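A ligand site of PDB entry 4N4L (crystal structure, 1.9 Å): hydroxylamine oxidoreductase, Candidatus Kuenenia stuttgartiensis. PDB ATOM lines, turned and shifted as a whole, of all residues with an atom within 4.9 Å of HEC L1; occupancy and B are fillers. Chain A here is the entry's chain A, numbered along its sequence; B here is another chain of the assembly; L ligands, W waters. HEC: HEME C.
NE2 of His 132 is bound to FE of HEC L1 (2.1 Å). An oxygen (O2A) of HEC L2 sits at hydrogen-bond distance from the backbone NH (N) of Ser 315 of chain B (2.8 Å). A ring nitrogen (NE2) of His 84 is bound to an iron atom (FE) of HEC L1 (2.1 Å). A carbon (CAB) of HEC L1 is bonded to the side-chain sulfur (SG) of Cys 80, 1.8 Å away. NE2 of His 128 is bound to FE of HEC L2, 2.1 Å away. NH1 of Arg 317 of chain B lies within salt-bridge range of O2A of HEC L1, at 2.9 Å. The backbone NH of Thr 71 is in hydrogen-bond range of an oxygen (O1D) of HEC L1 (3.0 Å). The side-chain sulfur (SG) of Cys 83 is bonded to a carbon (CAC) of HEC L1, at 1.8 Å. An oxygen (O1D) of HEC L1 lies within hydrogen-bond range of the backbone NH (N) of Gln 70 (3.0 Å). O1A of HEC L1 lies within hydrogen-bond range of OG of Ser 315 of chain B, 2.6 Å away. The side-chain sulfur (SG) of Cys 124 is covalently linked to a carbon (CAB) of HEC L2, 1.8 Å away. The side-chain hydroxyl (OG) of Ser 69 lies within hydrogen-bond range of an oxygen (O2D) of HEC L1, at 2.7 Å. OG1 of Thr 71 lies within hydrogen-bond range of O1D of HEC L1 (2.8 Å).
The backbone carbonyl oxygen (O) of Gly 68 lies close to the side-chain amide oxygen (OE1) of Gln 70 (3.0 Å). The side-chain amide oxygen of Gln 87 is in hydrogen-bond range of the side-chain amide nitrogen of Gln 311 of chain B (3.0 Å). A ring nitrogen (ND1) of His 132 lies within hydrogen-bond range of the backbone carbonyl oxygen (O) of Thr 71 (3.2 Å). A ring nitrogen (ND1) of His 132 lies within hydrogen-bond range of the side-chain hydroxyl (OG) of Ser 69. N of Lys 76 sits at hydrogen-bond distance from OE2 of Glu 79. OG of Ser 315 of chain B lies within hydrogen-bond range of N of Phe 318 of chain B, at 3.3 Å. The indole nitrogen (NE1) of Trp 65 sits at hydrogen-bond distance from the backbone carbonyl oxygen (O) of Leu 135. The backbone carbonyl oxygen of Phe 75 is in hydrogen-bond range of the side-chain amide nitrogen of Asn 130.
Trp 58 touches HEC L1. Trp 65 touches HEC L1 (CH2 to O2A, 3.4 Å). Phe 75 touches HEC L1 (CB to CBB, 3.7 Å). Glu 79 touches HEC L1 (O to CMC, 3.5 Å). Gln 87 touches HEC L1 (OE1 to CMD, 3.6 Å). O of Cys 124 touches CMB of HEC L1, at 3.5 Å. N of Ala 125 touches CMB of HEC L1 (3.7 Å). His 128 touches HEC L1 (CB to CMB, 3.7 Å). Gly 129 touches HEC L1. O of Asn 130 touches CBB of HEC L1, at 3.5 Å. Leu 135 touches HEC L1 (CD1 to C3A, 3.5 Å). Pro 316 of chain B touches HEC L1 (CD to CAD, 3.4 Å). Hydrophobic or aromatic side chains within 4 Å of HEC L1: Trp 58, Trp 65, Phe 75, His 84, Ala 125, His 128, His 132, Leu 135 and Pro 316 of chain B. 21 residues have an atom within 4 Å of HEC L1: Trp 58, Trp 65, Ser 69, Gln 70, Thr 71, Phe 75, Glu 79, Cys 80, Cys 83, His 84, Gln 87, Cys 124, Ala 125, His 128, Gly 129, Asn 130, His 132, Leu 135, Ser 315 of chain B, Pro 316 of chain B and Arg 317 of chain B. Along chain A the residues within 4 Å of HEC L1 span positions 58 to 135.
Water W1 lies within hydrogen-bond range of an oxygen (O2A) of HEC L1, the backbone NH (N) of Gly 68 and the guanidinium group (NH1) of Arg 317 of chain B. Water W3 bridges an oxygen (O2D) of HEC L1 (2.7 Å) and the side-chain hydroxyl (OG) of Ser 315 of chain B (3.4 Å).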
ATOM      1  N   TRP A  58     -17.070 -18.275   5.810  1.00  0.00           N
ATOM      2  CA  TRP A  58     -15.877 -19.036   5.402  1.00  0.00           C
ATOM      3  C   TRP A  58     -16.168 -20.520   5.218  1.00  0.00           C
ATOM      4  O   TRP A  58     -15.436 -21.206   4.509  1.00  0.00           O
ATOM      5  CB  TRP A  58     -14.729 -18.876   6.427  1.00  0.00           C
ATOM      6  CG  TRP A  58     -14.367 -17.454   6.679  1.00  0.00           C
ATOM      7  CD1 TRP A  58     -14.845 -16.654   7.679  1.00  0.00           C
ATOM      8  CD2 TRP A  58     -13.479 -16.649   5.911  1.00  0.00           C
ATOM      9  NE1 TRP A  58     -14.300 -15.404   7.579  1.00  0.00           N
ATOM     10  CE2 TRP A  58     -13.454 -15.365   6.501  1.00  0.00           C
ATOM     11  CE3 TRP A  58     -12.692 -16.876   4.779  1.00  0.00           C
ATOM     12  CZ2 TRP A  58     -12.684 -14.321   5.999  1.00  0.00           C
ATOM     13  CZ3 TRP A  58     -11.916 -15.840   4.276  1.00  0.00           C
ATOM     14  CH2 TRP A  58     -11.929 -14.573   4.876  1.00  0.00           C
ATOM     15  N   TRP A  65     -20.898 -16.204   1.491  1.00  0.00           N
ATOM     16  CA  TRP A  65     -19.705 -15.470   1.107  1.00  0.00           C
ATOM     17  C   TRP A  65     -20.057 -14.185   0.366  1.00  0.00           C
ATOM     18  O   TRP A  65     -20.878 -14.201  -0.560  1.00  0.00           O
ATOM     19  CB  TRP A  65     -18.770 -16.315   0.249  1.00  0.00           C
ATOM     20  CG  TRP A  65     -17.506 -15.610  -0.103  1.00  0.00           C
ATOM     21  CD1 TRP A  65     -17.158 -15.095  -1.330  1.00  0.00           C
ATOM     22  CD2 TRP A  65     -16.429 -15.284   0.779  1.00  0.00           C
ATOM     23  NE1 TRP A  65     -15.928 -14.500  -1.261  1.00  0.00           N
ATOM     24  CE2 TRP A  65     -15.453 -14.594   0.029  1.00  0.00           C
ATOM     25  CE3 TRP A  65     -16.186 -15.523   2.145  1.00  0.00           C
ATOM     26  CZ2 TRP A  65     -14.254 -14.147   0.586  1.00  0.00           C
ATOM     27  CZ3 TRP A  65     -14.994 -15.067   2.693  1.00  0.00           C
ATOM     28  CH2 TRP A  65     -14.044 -14.391   1.913  1.00  0.00           C
ATOM     29  N   GLY A  68     -15.463  -8.729   0.900  1.00  0.00           N
ATOM     30  CA  GLY A  68     -15.145  -7.906   2.060  1.00  0.00           C
ATOM     31  C   GLY A  68     -13.717  -7.399   2.051  1.00  0.00           C
ATOM     32  O   GLY A  68     -13.145  -7.115   3.105  1.00  0.00           O
ATOM     33  N   SER A  69     -13.141  -7.266   0.865  1.00  0.00           N
ATOM     34  CA  SER A  69     -11.759  -6.841   0.706  1.00  0.00           C
ATOM     35  C   SER A  69     -11.699  -5.343   0.433  1.00  0.00           C
ATOM     36  O   SER A  69     -12.634  -4.754  -0.114  1.00  0.00           O
ATOM     37  CB  SER A  69     -11.097  -7.610  -0.435  1.00  0.00           C
ATOM     38  OG  SER A  69      -9.781  -7.160  -0.656  1.00  0.00           O
ATOM     39  N   GLN A  70     -10.593  -4.718   0.829  1.00  0.00           N
ATOM     40  CA  GLN A  70     -10.368  -3.290   0.585  1.00  0.00           C
ATOM     41  C   GLN A  70      -9.431  -3.068  -0.605  1.00  0.00           C
ATOM     42  O   GLN A  70      -9.238  -1.933  -1.042  1.00  0.00           O
ATOM     43  CB  GLN A  70      -9.781  -2.625   1.844  1.00  0.00           C
ATOM     44  CG  GLN A  70     -10.743  -2.584   3.033  1.00  0.00           C
ATOM     45  CD  GLN A  70     -11.023  -3.959   3.634  1.00  0.00           C
ATOM     46  OE1 GLN A  70     -12.172  -4.331   3.854  1.00  0.00           O
ATOM     47  NE2 GLN A  70      -9.965  -4.726   3.883  1.00  0.00           N
ATOM     48  N   THR A  71      -8.837  -4.144  -1.117  1.00  0.00           N
ATOM     49  CA  THR A  71      -7.895  -4.065  -2.216  1.00  0.00           C
ATOM     50  C   THR A  71      -8.642  -4.239  -3.535  1.00  0.00           C
ATOM     51  O   THR A  71      -9.454  -5.162  -3.672  1.00  0.00           O
ATOM     52  CB  THR A  71      -6.790  -5.134  -2.065  1.00  0.00           C
ATOM     53  OG1 THR A  71      -6.052  -4.893  -0.857  1.00  0.00           O
ATOM     54  CG2 THR A  71      -5.822  -5.135  -3.238  1.00  0.00           C
ATOM     55  N   PHE A  75      -5.832  -8.973 -11.309  1.00  0.00           N
ATOM     56  CA  PHE A  75      -4.415  -9.340 -11.281  1.00  0.00           C
ATOM     57  C   PHE A  75      -4.143 -10.697 -11.902  1.00  0.00           C
ATOM     58  O   PHE A  75      -5.010 -11.572 -11.917  1.00  0.00           O
ATOM     59  CB  PHE A  75      -3.918  -9.373  -9.832  1.00  0.00           C
ATOM     60  CG  PHE A  75      -4.073  -8.077  -9.097  1.00  0.00           C
ATOM     61  CD1 PHE A  75      -3.281  -6.988  -9.421  1.00  0.00           C
ATOM     62  CD2 PHE A  75      -5.002  -7.938  -8.079  1.00  0.00           C
ATOM     63  CE1 PHE A  75      -3.416  -5.779  -8.750  1.00  0.00           C
ATOM     64  CE2 PHE A  75      -5.144  -6.737  -7.398  1.00  0.00           C
ATOM     65  CZ  PHE A  75      -4.348  -5.653  -7.743  1.00  0.00           C
ATOM     66  N   LYS A  76      -2.914 -10.876 -12.391  1.00  0.00           N
ATOM     67  CA  LYS A  76      -2.429 -12.174 -12.857  1.00  0.00           C
ATOM     68  C   LYS A  76      -1.909 -12.946 -11.658  1.00  0.00           C
ATOM     69  O   LYS A  76      -1.517 -12.342 -10.657  1.00  0.00           O
ATOM     70  CB  LYS A  76      -1.301 -11.980 -13.871  1.00  0.00           C
ATOM     71  CG  LYS A  76      -1.681 -11.157 -15.102  1.00  0.00           C
ATOM     72  CD  LYS A  76      -0.457 -10.771 -15.934  1.00  0.00           C
ATOM     73  CE  LYS A  76      -0.870  -9.971 -17.177  1.00  0.00           C
ATOM     74  NZ  LYS A  76       0.284  -9.750 -18.098  1.00  0.00           N
ATOM     75  N   GLU A  79       1.147 -11.695  -9.902  1.00  0.00           N
ATOM     76  CA  GLU A  79       0.923 -10.491  -9.104  1.00  0.00           C
ATOM     77  C   GLU A  79       0.317 -10.824  -7.741  1.00  0.00           C
ATOM     78  O   GLU A  79       0.693 -10.233  -6.740  1.00  0.00           O
ATOM     79  CB  GLU A  79       0.053  -9.499  -9.881  1.00  0.00           C
ATOM     80  CG  GLU A  79       0.749  -8.976 -11.141  1.00  0.00           C
ATOM     81  CD  GLU A  79      -0.146  -8.190 -12.067  1.00  0.00           C
ATOM     82  OE1 GLU A  79       0.412  -7.397 -12.843  1.00  0.00           O
ATOM     83  OE2 GLU A  79      -1.383  -8.370 -12.056  1.00  0.00           O
ATOM     84  N   CYS A  80      -0.614 -11.782  -7.713  1.00  0.00           N
ATOM     85  CA  CYS A  80      -1.116 -12.312  -6.437  1.00  0.00           C
ATOM     86  C   CYS A  80       0.047 -12.706  -5.533  1.00  0.00           C
ATOM     87  O   CYS A  80       0.082 -12.337  -4.358  1.00  0.00           O
ATOM     88  CB  CYS A  80      -1.982 -13.572  -6.638  1.00  0.00           C
ATOM     89  SG  CYS A  80      -3.296 -13.489  -7.860  1.00  0.00           S
ATOM     90  N   CYS A  83       2.537  -9.680  -4.148  1.00  0.00           N
ATOM     91  CA  CYS A  83       1.981  -8.864  -3.079  1.00  0.00           C
ATOM     92  C   CYS A  83       1.736  -9.679  -1.812  1.00  0.00           C
ATOM     93  O   CYS A  83       2.022  -9.204  -0.710  1.00  0.00           O
ATOM     94  CB  CYS A  83       0.691  -8.212  -3.530  1.00  0.00           C
ATOM     95  SG  CYS A  83       0.100  -6.995  -2.360  1.00  0.00           S
ATOM     96  N   HIS A  84       1.210 -10.891  -1.960  1.00  0.00           N
ATOM     97  CA  HIS A  84       0.959 -11.741  -0.799  1.00  0.00           C
ATOM     98  C   HIS A  84       2.216 -12.280  -0.146  1.00  0.00           C
ATOM     99  O   HIS A  84       2.173 -12.710   1.000  1.00  0.00           O
ATOM    100  CB  HIS A  84      -0.032 -12.866  -1.134  1.00  0.00           C
ATOM    101  CG  HIS A  84      -1.450 -12.420  -1.050  1.00  0.00           C
ATOM    102  ND1 HIS A  84      -2.174 -12.474   0.129  1.00  0.00           N
ATOM    103  CD2 HIS A  84      -2.263 -11.855  -1.963  1.00  0.00           C
ATOM    104  CE1 HIS A  84      -3.375 -11.968  -0.077  1.00  0.00           C
ATOM    105  NE2 HIS A  84      -3.462 -11.592  -1.333  1.00  0.00           N
ATOM    106  N   GLN A  87       2.137  -9.538   2.171  1.00  0.00           N
ATOM    107  CA  GLN A  87       0.907  -9.340   2.946  1.00  0.00           C
ATOM    108  C   GLN A  87       0.416 -10.548   3.748  1.00  0.00           C
ATOM    109  O   GLN A  87      -0.167 -10.371   4.828  1.00  0.00           O
ATOM    110  CB  GLN A  87      -0.204  -8.814   2.028  1.00  0.00           C
ATOM    111  CG  GLN A  87       0.017  -7.355   1.615  1.00  0.00           C
ATOM    112  CD  GLN A  87       0.009  -6.421   2.805  1.00  0.00           C
ATOM    113  OE1 GLN A  87      -0.759  -6.604   3.755  1.00  0.00           O
ATOM    114  NE2 GLN A  87       0.875  -5.396   2.770  1.00  0.00           N
ATOM    115  N   CYS A 124      -2.974 -18.593  -7.163  1.00  0.00           N
ATOM    116  CA  CYS A 124      -3.979 -17.970  -6.302  1.00  0.00           C
ATOM    117  C   CYS A 124      -5.246 -17.644  -7.077  1.00  0.00           C
ATOM    118  O   CYS A 124      -6.355 -17.883  -6.597  1.00  0.00           O
ATOM    119  CB  CYS A 124      -3.450 -16.672  -5.676  1.00  0.00           C
ATOM    120  SG  CYS A 124      -1.759 -16.706  -5.032  1.00  0.00           S
ATOM    121  N   ALA A 125      -5.076 -17.079  -8.283  1.00  0.00           N
ATOM    122  CA  ALA A 125      -6.202 -16.622  -9.099  1.00  0.00           C
ATOM    123  C   ALA A 125      -7.010 -17.790  -9.666  1.00  0.00           C
ATOM    124  O   ALA A 125      -8.216 -17.653  -9.905  1.00  0.00           O
ATOM    125  CB  ALA A 125      -5.711 -15.707 -10.237  1.00  0.00           C
ATOM    126  N   HIS A 128      -9.127 -18.597  -6.543  1.00  0.00           N
ATOM    127  CA  HIS A 128      -9.864 -17.508  -5.877  1.00  0.00           C
ATOM    128  C   HIS A 128     -10.453 -16.446  -6.805  1.00  0.00           C
ATOM    129  O   HIS A 128     -11.151 -15.545  -6.331  1.00  0.00           O
ATOM    130  CB  HIS A 128      -8.939 -16.827  -4.861  1.00  0.00           C
ATOM    131  CG  HIS A 128      -8.604 -17.685  -3.693  1.00  0.00           C
ATOM    132  ND1 HIS A 128      -9.528 -17.994  -2.719  1.00  0.00           N
ATOM    133  CD2 HIS A 128      -7.463 -18.318  -3.339  1.00  0.00           C
ATOM    134  CE1 HIS A 128      -8.964 -18.775  -1.819  1.00  0.00           C
ATOM    135  NE2 HIS A 128      -7.713 -18.990  -2.173  1.00  0.00           N
ATOM    136  N   GLY A 129     -10.156 -16.535  -8.095  1.00  0.00           N
ATOM    137  CA  GLY A 129     -10.544 -15.504  -9.053  1.00  0.00           C
ATOM    138  C   GLY A 129      -9.462 -14.442  -9.199  1.00  0.00           C
ATOM    139  O   GLY A 129      -8.561 -14.360  -8.360  1.00  0.00           O
ATOM    140  N   ASN A 130      -9.560 -13.650 -10.273  1.00  0.00           N
ATOM    141  CA  ASN A 130      -8.571 -12.619 -10.629  1.00  0.00           C
ATOM    142  C   ASN A 130      -8.903 -11.229 -10.090  1.00  0.00           C
ATOM    143  O   ASN A 130      -8.007 -10.402  -9.913  1.00  0.00           O
ATOM    144  CB  ASN A 130      -8.451 -12.516 -12.152  1.00  0.00           C
ATOM    145  CG  ASN A 130      -7.873 -13.761 -12.779  1.00  0.00           C
ATOM    146  OD1 ASN A 130      -8.602 -14.608 -13.296  1.00  0.00           O
ATOM    147  ND2 ASN A 130      -6.548 -13.878 -12.759  1.00  0.00           N
ATOM    148  N   HIS A 132      -9.954  -8.673  -7.346  1.00  0.00           N
ATOM    149  CA  HIS A 132      -9.805  -8.630  -5.891  1.00  0.00           C
ATOM    150  C   HIS A 132     -11.061  -8.150  -5.155  1.00  0.00           C
ATOM    151  O   HIS A 132     -11.144  -8.255  -3.928  1.00  0.00           O
ATOM    152  CB  HIS A 132      -8.600  -7.790  -5.481  1.00  0.00           C
ATOM    153  CG  HIS A 132      -7.919  -8.314  -4.258  1.00  0.00           C
ATOM    154  ND1 HIS A 132      -8.417  -8.109  -2.987  1.00  0.00           N
ATOM    155  CD2 HIS A 132      -6.820  -9.079  -4.113  1.00  0.00           C
ATOM    156  CE1 HIS A 132      -7.626  -8.709  -2.108  1.00  0.00           C
ATOM    157  NE2 HIS A 132      -6.649  -9.305  -2.770  1.00  0.00           N
ATOM    158  N   LEU A 135     -13.438 -11.893  -5.082  1.00  0.00           N
ATOM    159  CA  LEU A 135     -12.688 -13.085  -4.731  1.00  0.00           C
ATOM    160  C   LEU A 135     -13.649 -14.188  -4.295  1.00  0.00           C
ATOM    161  O   LEU A 135     -14.728 -13.912  -3.773  1.00  0.00           O
ATOM    162  CB  LEU A 135     -11.674 -12.804  -3.618  1.00  0.00           C
ATOM    163  CG  LEU A 135     -10.525 -11.880  -4.032  1.00  0.00           C
ATOM    164  CD1 LEU A 135      -9.773 -11.363  -2.805  1.00  0.00           C
ATOM    165  CD2 LEU A 135      -9.558 -12.564  -5.000  1.00  0.00           C
ATOM    166  N   MET A 137     -14.359 -17.918  -2.303  1.00  0.00           N
ATOM    167  CA  MET A 137     -13.947 -18.759  -1.178  1.00  0.00           C
ATOM    168  C   MET A 137     -14.502 -20.156  -1.472  1.00  0.00           C
ATOM    169  O   MET A 137     -15.702 -20.390  -1.370  1.00  0.00           O
ATOM    170  CB  MET A 137     -14.474 -18.174   0.129  1.00  0.00           C
ATOM    171  CG  MET A 137     -13.748 -18.642   1.377  1.00  0.00           C
ATOM    172  SD  MET A 137     -11.936 -18.566   1.300  1.00  0.00           S
ATOM    173  CE  MET A 137     -11.608 -16.881   0.811  1.00  0.00           C
ATOM    174  N   GLN B 311      -2.293 -12.183  10.440  1.00  0.00           N
ATOM    175  CA  GLN B 311      -2.107 -11.907   9.019  1.00  0.00           C
ATOM    176  C   GLN B 311      -0.731 -12.324   8.495  1.00  0.00           C
ATOM    177  O   GLN B 311      -0.511 -12.334   7.283  1.00  0.00           O
ATOM    178  CB  GLN B 311      -2.381 -10.417   8.707  1.00  0.00           C
ATOM    179  CG  GLN B 311      -2.579 -10.130   7.203  1.00  0.00           C
ATOM    180  CD  GLN B 311      -2.741  -8.653   6.881  1.00  0.00           C
ATOM    181  OE1 GLN B 311      -3.262  -7.886   7.688  1.00  0.00           O
ATOM    182  NE2 GLN B 311      -2.298  -8.249   5.683  1.00  0.00           N
ATOM    183  N   SER B 315      -5.790 -14.163   5.946  1.00  0.00           N
ATOM    184  CA  SER B 315      -6.558 -12.952   5.690  1.00  0.00           C
ATOM    185  C   SER B 315      -6.848 -12.249   7.008  1.00  0.00           C
ATOM    186  O   SER B 315      -7.193 -12.918   7.989  1.00  0.00           O
ATOM    187  CB  SER B 315      -7.885 -13.325   5.032  1.00  0.00           C
ATOM    188  OG  SER B 315      -8.836 -12.293   5.219  1.00  0.00           O
ATOM    189  N   PRO B 316      -6.730 -10.909   7.042  1.00  0.00           N
ATOM    190  CA  PRO B 316      -7.083 -10.185   8.266  1.00  0.00           C
ATOM    191  C   PRO B 316      -8.585 -10.214   8.541  1.00  0.00           C
ATOM    192  O   PRO B 316      -9.001 -10.061   9.686  1.00  0.00           O
ATOM    193  CB  PRO B 316      -6.619  -8.754   7.974  1.00  0.00           C
ATOM    194  CG  PRO B 316      -6.655  -8.629   6.505  1.00  0.00           C
ATOM    195  CD  PRO B 316      -6.328  -9.996   5.960  1.00  0.00           C
ATOM    196  N   ARG B 317      -9.381 -10.404   7.496  1.00  0.00           N
ATOM    197  CA  ARG B 317     -10.835 -10.524   7.643  1.00  0.00           C
ATOM    198  C   ARG B 317     -11.159 -11.830   8.369  1.00  0.00           C
ATOM    199  O   ARG B 317     -11.985 -11.870   9.272  1.00  0.00           O
ATOM    200  CB  ARG B 317     -11.491 -10.501   6.265  1.00  0.00           C
ATOM    201  CG  ARG B 317     -13.004 -10.420   6.273  1.00  0.00           C
ATOM    202  CD  ARG B 317     -13.519 -10.629   4.872  1.00  0.00           C
ATOM    203  NE  ARG B 317     -14.969 -10.543   4.775  1.00  0.00           N
ATOM    204  CZ  ARG B 317     -15.666 -10.893   3.690  1.00  0.00           C
ATOM    205  NH1 ARG B 317     -15.046 -11.348   2.607  1.00  0.00           N
ATOM    206  NH2 ARG B 317     -16.983 -10.772   3.680  1.00  0.00           N
ATOM    207  N   PHE B 318     -10.500 -12.914   7.952  1.00  0.00           N
ATOM    208  CA  PHE B 318     -10.626 -14.198   8.626  1.00  0.00           C
ATOM    209  C   PHE B 318     -10.226 -14.105  10.100  1.00  0.00           C
ATOM    210  O   PHE B 318     -10.972 -14.543  10.991  1.00  0.00           O
ATOM    211  CB  PHE B 318      -9.780 -15.245   7.917  1.00  0.00           C
ATOM    212  CG  PHE B 318      -9.842 -16.610   8.545  1.00  0.00           C
ATOM    213  CD1 PHE B 318     -11.046 -17.282   8.644  1.00  0.00           C
ATOM    214  CD2 PHE B 318      -8.695 -17.194   9.057  1.00  0.00           C
ATOM    215  CE1 PHE B 318     -11.104 -18.535   9.237  1.00  0.00           C
ATOM    216  CE2 PHE B 318      -8.740 -18.447   9.638  1.00  0.00           C
ATOM    217  CZ  PHE B 318      -9.944 -19.118   9.728  1.00  0.00           C
HETATM  218 FE   HEC L   1      -5.005 -10.428  -2.118  1.00  0.00          FE
HETATM  219  CHA HEC L   1      -6.772 -10.400   0.818  1.00  0.00           C
HETATM  220  CHB HEC L   1      -6.312 -13.468  -2.881  1.00  0.00           C
HETATM  221  CHC HEC L   1      -3.758 -10.129  -5.304  1.00  0.00           C
HETATM  222  CHD HEC L   1      -3.206  -7.713  -1.154  1.00  0.00           C
HETATM  223  NA  HEC L   1      -6.291 -11.726  -1.192  1.00  0.00           N
HETATM  224  C1A HEC L   1      -6.957 -11.479  -0.014  1.00  0.00           C
HETATM  225  C2A HEC L   1      -7.865 -12.576   0.216  1.00  0.00           C
HETATM  226  C3A HEC L   1      -7.747 -13.449  -0.790  1.00  0.00           C
HETATM  227  C4A HEC L   1      -6.747 -12.913  -1.706  1.00  0.00           C
HETATM  228  CMA HEC L   1      -8.533 -14.765  -0.975  1.00  0.00           C
HETATM  229  CAA HEC L   1      -8.813 -12.669   1.425  1.00  0.00           C
HETATM  230  CBA HEC L   1      -9.998 -11.765   1.083  1.00  0.00           C
HETATM  231  CGA HEC L   1     -10.992 -11.646   2.204  1.00  0.00           C
HETATM  232  O1A HEC L   1     -10.584 -11.631   3.393  1.00  0.00           O
HETATM  233  O2A HEC L   1     -12.217 -11.563   1.909  1.00  0.00           O
HETATM  234  NB  HEC L   1      -4.986 -11.584  -3.756  1.00  0.00           N
HETATM  235  C1B HEC L   1      -5.668 -12.791  -3.892  1.00  0.00           C
HETATM  236  C2B HEC L   1      -5.599 -13.204  -5.274  1.00  0.00           C
HETATM  237  C3B HEC L   1      -4.893 -12.282  -5.930  1.00  0.00           C
HETATM  238  C4B HEC L   1      -4.492 -11.258  -5.010  1.00  0.00           C
HETATM  239  CMB HEC L   1      -6.229 -14.488  -5.850  1.00  0.00           C
HETATM  240  CAB HEC L   1      -4.563 -12.289  -7.433  1.00  0.00           C
HETATM  241  CBB HEC L   1      -5.589 -12.337  -8.289  1.00  0.00           C
HETATM  242  NC  HEC L   1      -3.730  -9.150  -3.047  1.00  0.00           N
HETATM  243  C1C HEC L   1      -3.340  -9.211  -4.370  1.00  0.00           C
HETATM  244  C2C HEC L   1      -2.409  -8.144  -4.616  1.00  0.00           C
HETATM  245  C3C HEC L   1      -2.244  -7.465  -3.466  1.00  0.00           C
HETATM  246  C4C HEC L   1      -3.084  -8.099  -2.465  1.00  0.00           C
HETATM  247  CMC HEC L   1      -1.747  -7.883  -5.983  1.00  0.00           C
HETATM  248  CAC HEC L   1      -1.321  -6.250  -3.204  1.00  0.00           C
HETATM  249  CBC HEC L   1      -0.988  -5.433  -4.203  1.00  0.00           C
HETATM  250  ND  HEC L   1      -4.997  -9.246  -0.438  1.00  0.00           N
HETATM  251  C1D HEC L   1      -4.141  -8.168  -0.262  1.00  0.00           C
HETATM  252  C2D HEC L   1      -4.382  -7.577   1.036  1.00  0.00           C
HETATM  253  C3D HEC L   1      -5.495  -8.410   1.653  1.00  0.00           C
HETATM  254  C4D HEC L   1      -5.813  -9.423   0.678  1.00  0.00           C
HETATM  255  CMD HEC L   1      -3.682  -6.353   1.670  1.00  0.00           C
HETATM  256  CAD HEC L   1      -6.130  -8.181   3.038  1.00  0.00           C
HETATM  257  CBD HEC L   1      -6.858  -6.839   3.052  1.00  0.00           C
HETATM  258  CGD HEC L   1      -7.827  -6.733   1.900  1.00  0.00           C
HETATM  259  O1D HEC L   1      -7.829  -5.676   1.223  1.00  0.00           O
HETATM  260  O2D HEC L   1      -8.597  -7.705   1.662  1.00  0.00           O
HETATM  261 FE   HEC L   2      -6.273 -19.940  -0.995  1.00  0.00          FE
HETATM  262  CHA HEC L   2      -8.477 -19.933   1.625  1.00  0.00           C
HETATM  263  CHB HEC L   2      -5.274 -16.797  -0.216  1.00  0.00           C
HETATM  264  CHC HEC L   2      -3.748 -20.184  -3.307  1.00  0.00           C
HETATM  265  CHD HEC L   2      -7.658 -22.786  -2.260  1.00  0.00           C
HETATM  266  NA  HEC L   2      -6.782 -18.613   0.449  1.00  0.00           N
HETATM  267  C1A HEC L   2      -7.717 -18.794   1.442  1.00  0.00           C
HETATM  268  C2A HEC L   2      -7.734 -17.600   2.264  1.00  0.00           C
HETATM  269  C3A HEC L   2      -6.851 -16.735   1.749  1.00  0.00           C
HETATM  270  C4A HEC L   2      -6.222 -17.363   0.601  1.00  0.00           C
HETATM  271  CMA HEC L   2      -6.509 -15.319   2.274  1.00  0.00           C
HETATM  272  CAA HEC L   2      -8.651 -17.389   3.485  1.00  0.00           C
HETATM  273  CBA HEC L   2      -8.323 -18.351   4.629  1.00  0.00           C
HETATM  274  CGA HEC L   2      -7.130 -17.877   5.412  1.00  0.00           C
HETATM  275  O1A HEC L   2      -6.369 -18.746   5.921  1.00  0.00           O
HETATM  276  O2A HEC L   2      -6.951 -16.638   5.549  1.00  0.00           O
HETATM  277  NB  HEC L   2      -4.801 -18.718  -1.652  1.00  0.00           N
HETATM  278  C1B HEC L   2      -4.552 -17.440  -1.181  1.00  0.00           C
HETATM  279  C2B HEC L   2      -3.378 -16.930  -1.869  1.00  0.00           C
HETATM  280  C3B HEC L   2      -2.969 -17.878  -2.715  1.00  0.00           C
HETATM  281  C4B HEC L   2      -3.850 -19.021  -2.594  1.00  0.00           C
HETATM  282  CMB HEC L   2      -2.745 -15.531  -1.661  1.00  0.00           C
HETATM  283  CAB HEC L   2      -1.750 -17.825  -3.634  1.00  0.00           C
HETATM  284  CBB HEC L   2      -0.541 -17.720  -3.057  1.00  0.00           C
HETATM  285  NC  HEC L   2      -5.761 -21.269  -2.490  1.00  0.00           N
HETATM  286  C1C HEC L   2      -4.737 -21.126  -3.393  1.00  0.00           C
HETATM  287  C2C HEC L   2      -4.895 -22.132  -4.419  1.00  0.00           C
HETATM  288  C3C HEC L   2      -5.986 -22.845  -4.130  1.00  0.00           C
HETATM  289  C4C HEC L   2      -6.542 -22.316  -2.910  1.00  0.00           C
HETATM  290  CMC HEC L   2      -3.959 -22.318  -5.627  1.00  0.00           C
HETATM  291  CAC HEC L   2      -6.562 -24.006  -4.977  1.00  0.00           C
HETATM  292  CBC HEC L   2      -5.813 -25.102  -5.179  1.00  0.00           C
HETATM  293  ND  HEC L   2      -7.780 -21.180  -0.388  1.00  0.00           N
HETATM  294  C1D HEC L   2      -8.208 -22.277  -1.114  1.00  0.00           C
HETATM  295  C2D HEC L   2      -9.380 -22.836  -0.494  1.00  0.00           C
HETATM  296  C3D HEC L   2      -9.651 -21.956   0.717  1.00  0.00           C
HETATM  297  C4D HEC L   2      -8.612 -20.941   0.698  1.00  0.00           C
HETATM  298  CMD HEC L   2     -10.200 -24.061  -0.947  1.00  0.00           C
HETATM  299  CAD HEC L   2     -10.819 -22.111   1.699  1.00  0.00           C
HETATM  300  CBD HEC L   2     -10.402 -22.659   3.049  1.00  0.00           C
HETATM  301  CGD HEC L   2     -10.140 -24.146   2.977  1.00  0.00           C
HETATM  302  O1D HEC L   2      -9.301 -24.607   3.792  1.00  0.00           O
HETATM  303  O2D HEC L   2     -10.753 -24.865   2.146  1.00  0.00           O
HETATM  304  O   HOH W   1     -13.548 -10.592  -0.165  1.00  0.00           O
HETATM  305  O   HOH W   2      -2.145  -3.886   2.920  1.00  0.00           O
HETATM  306  O   HOH W   3      -9.289  -9.200   3.825  1.00  0.00           O
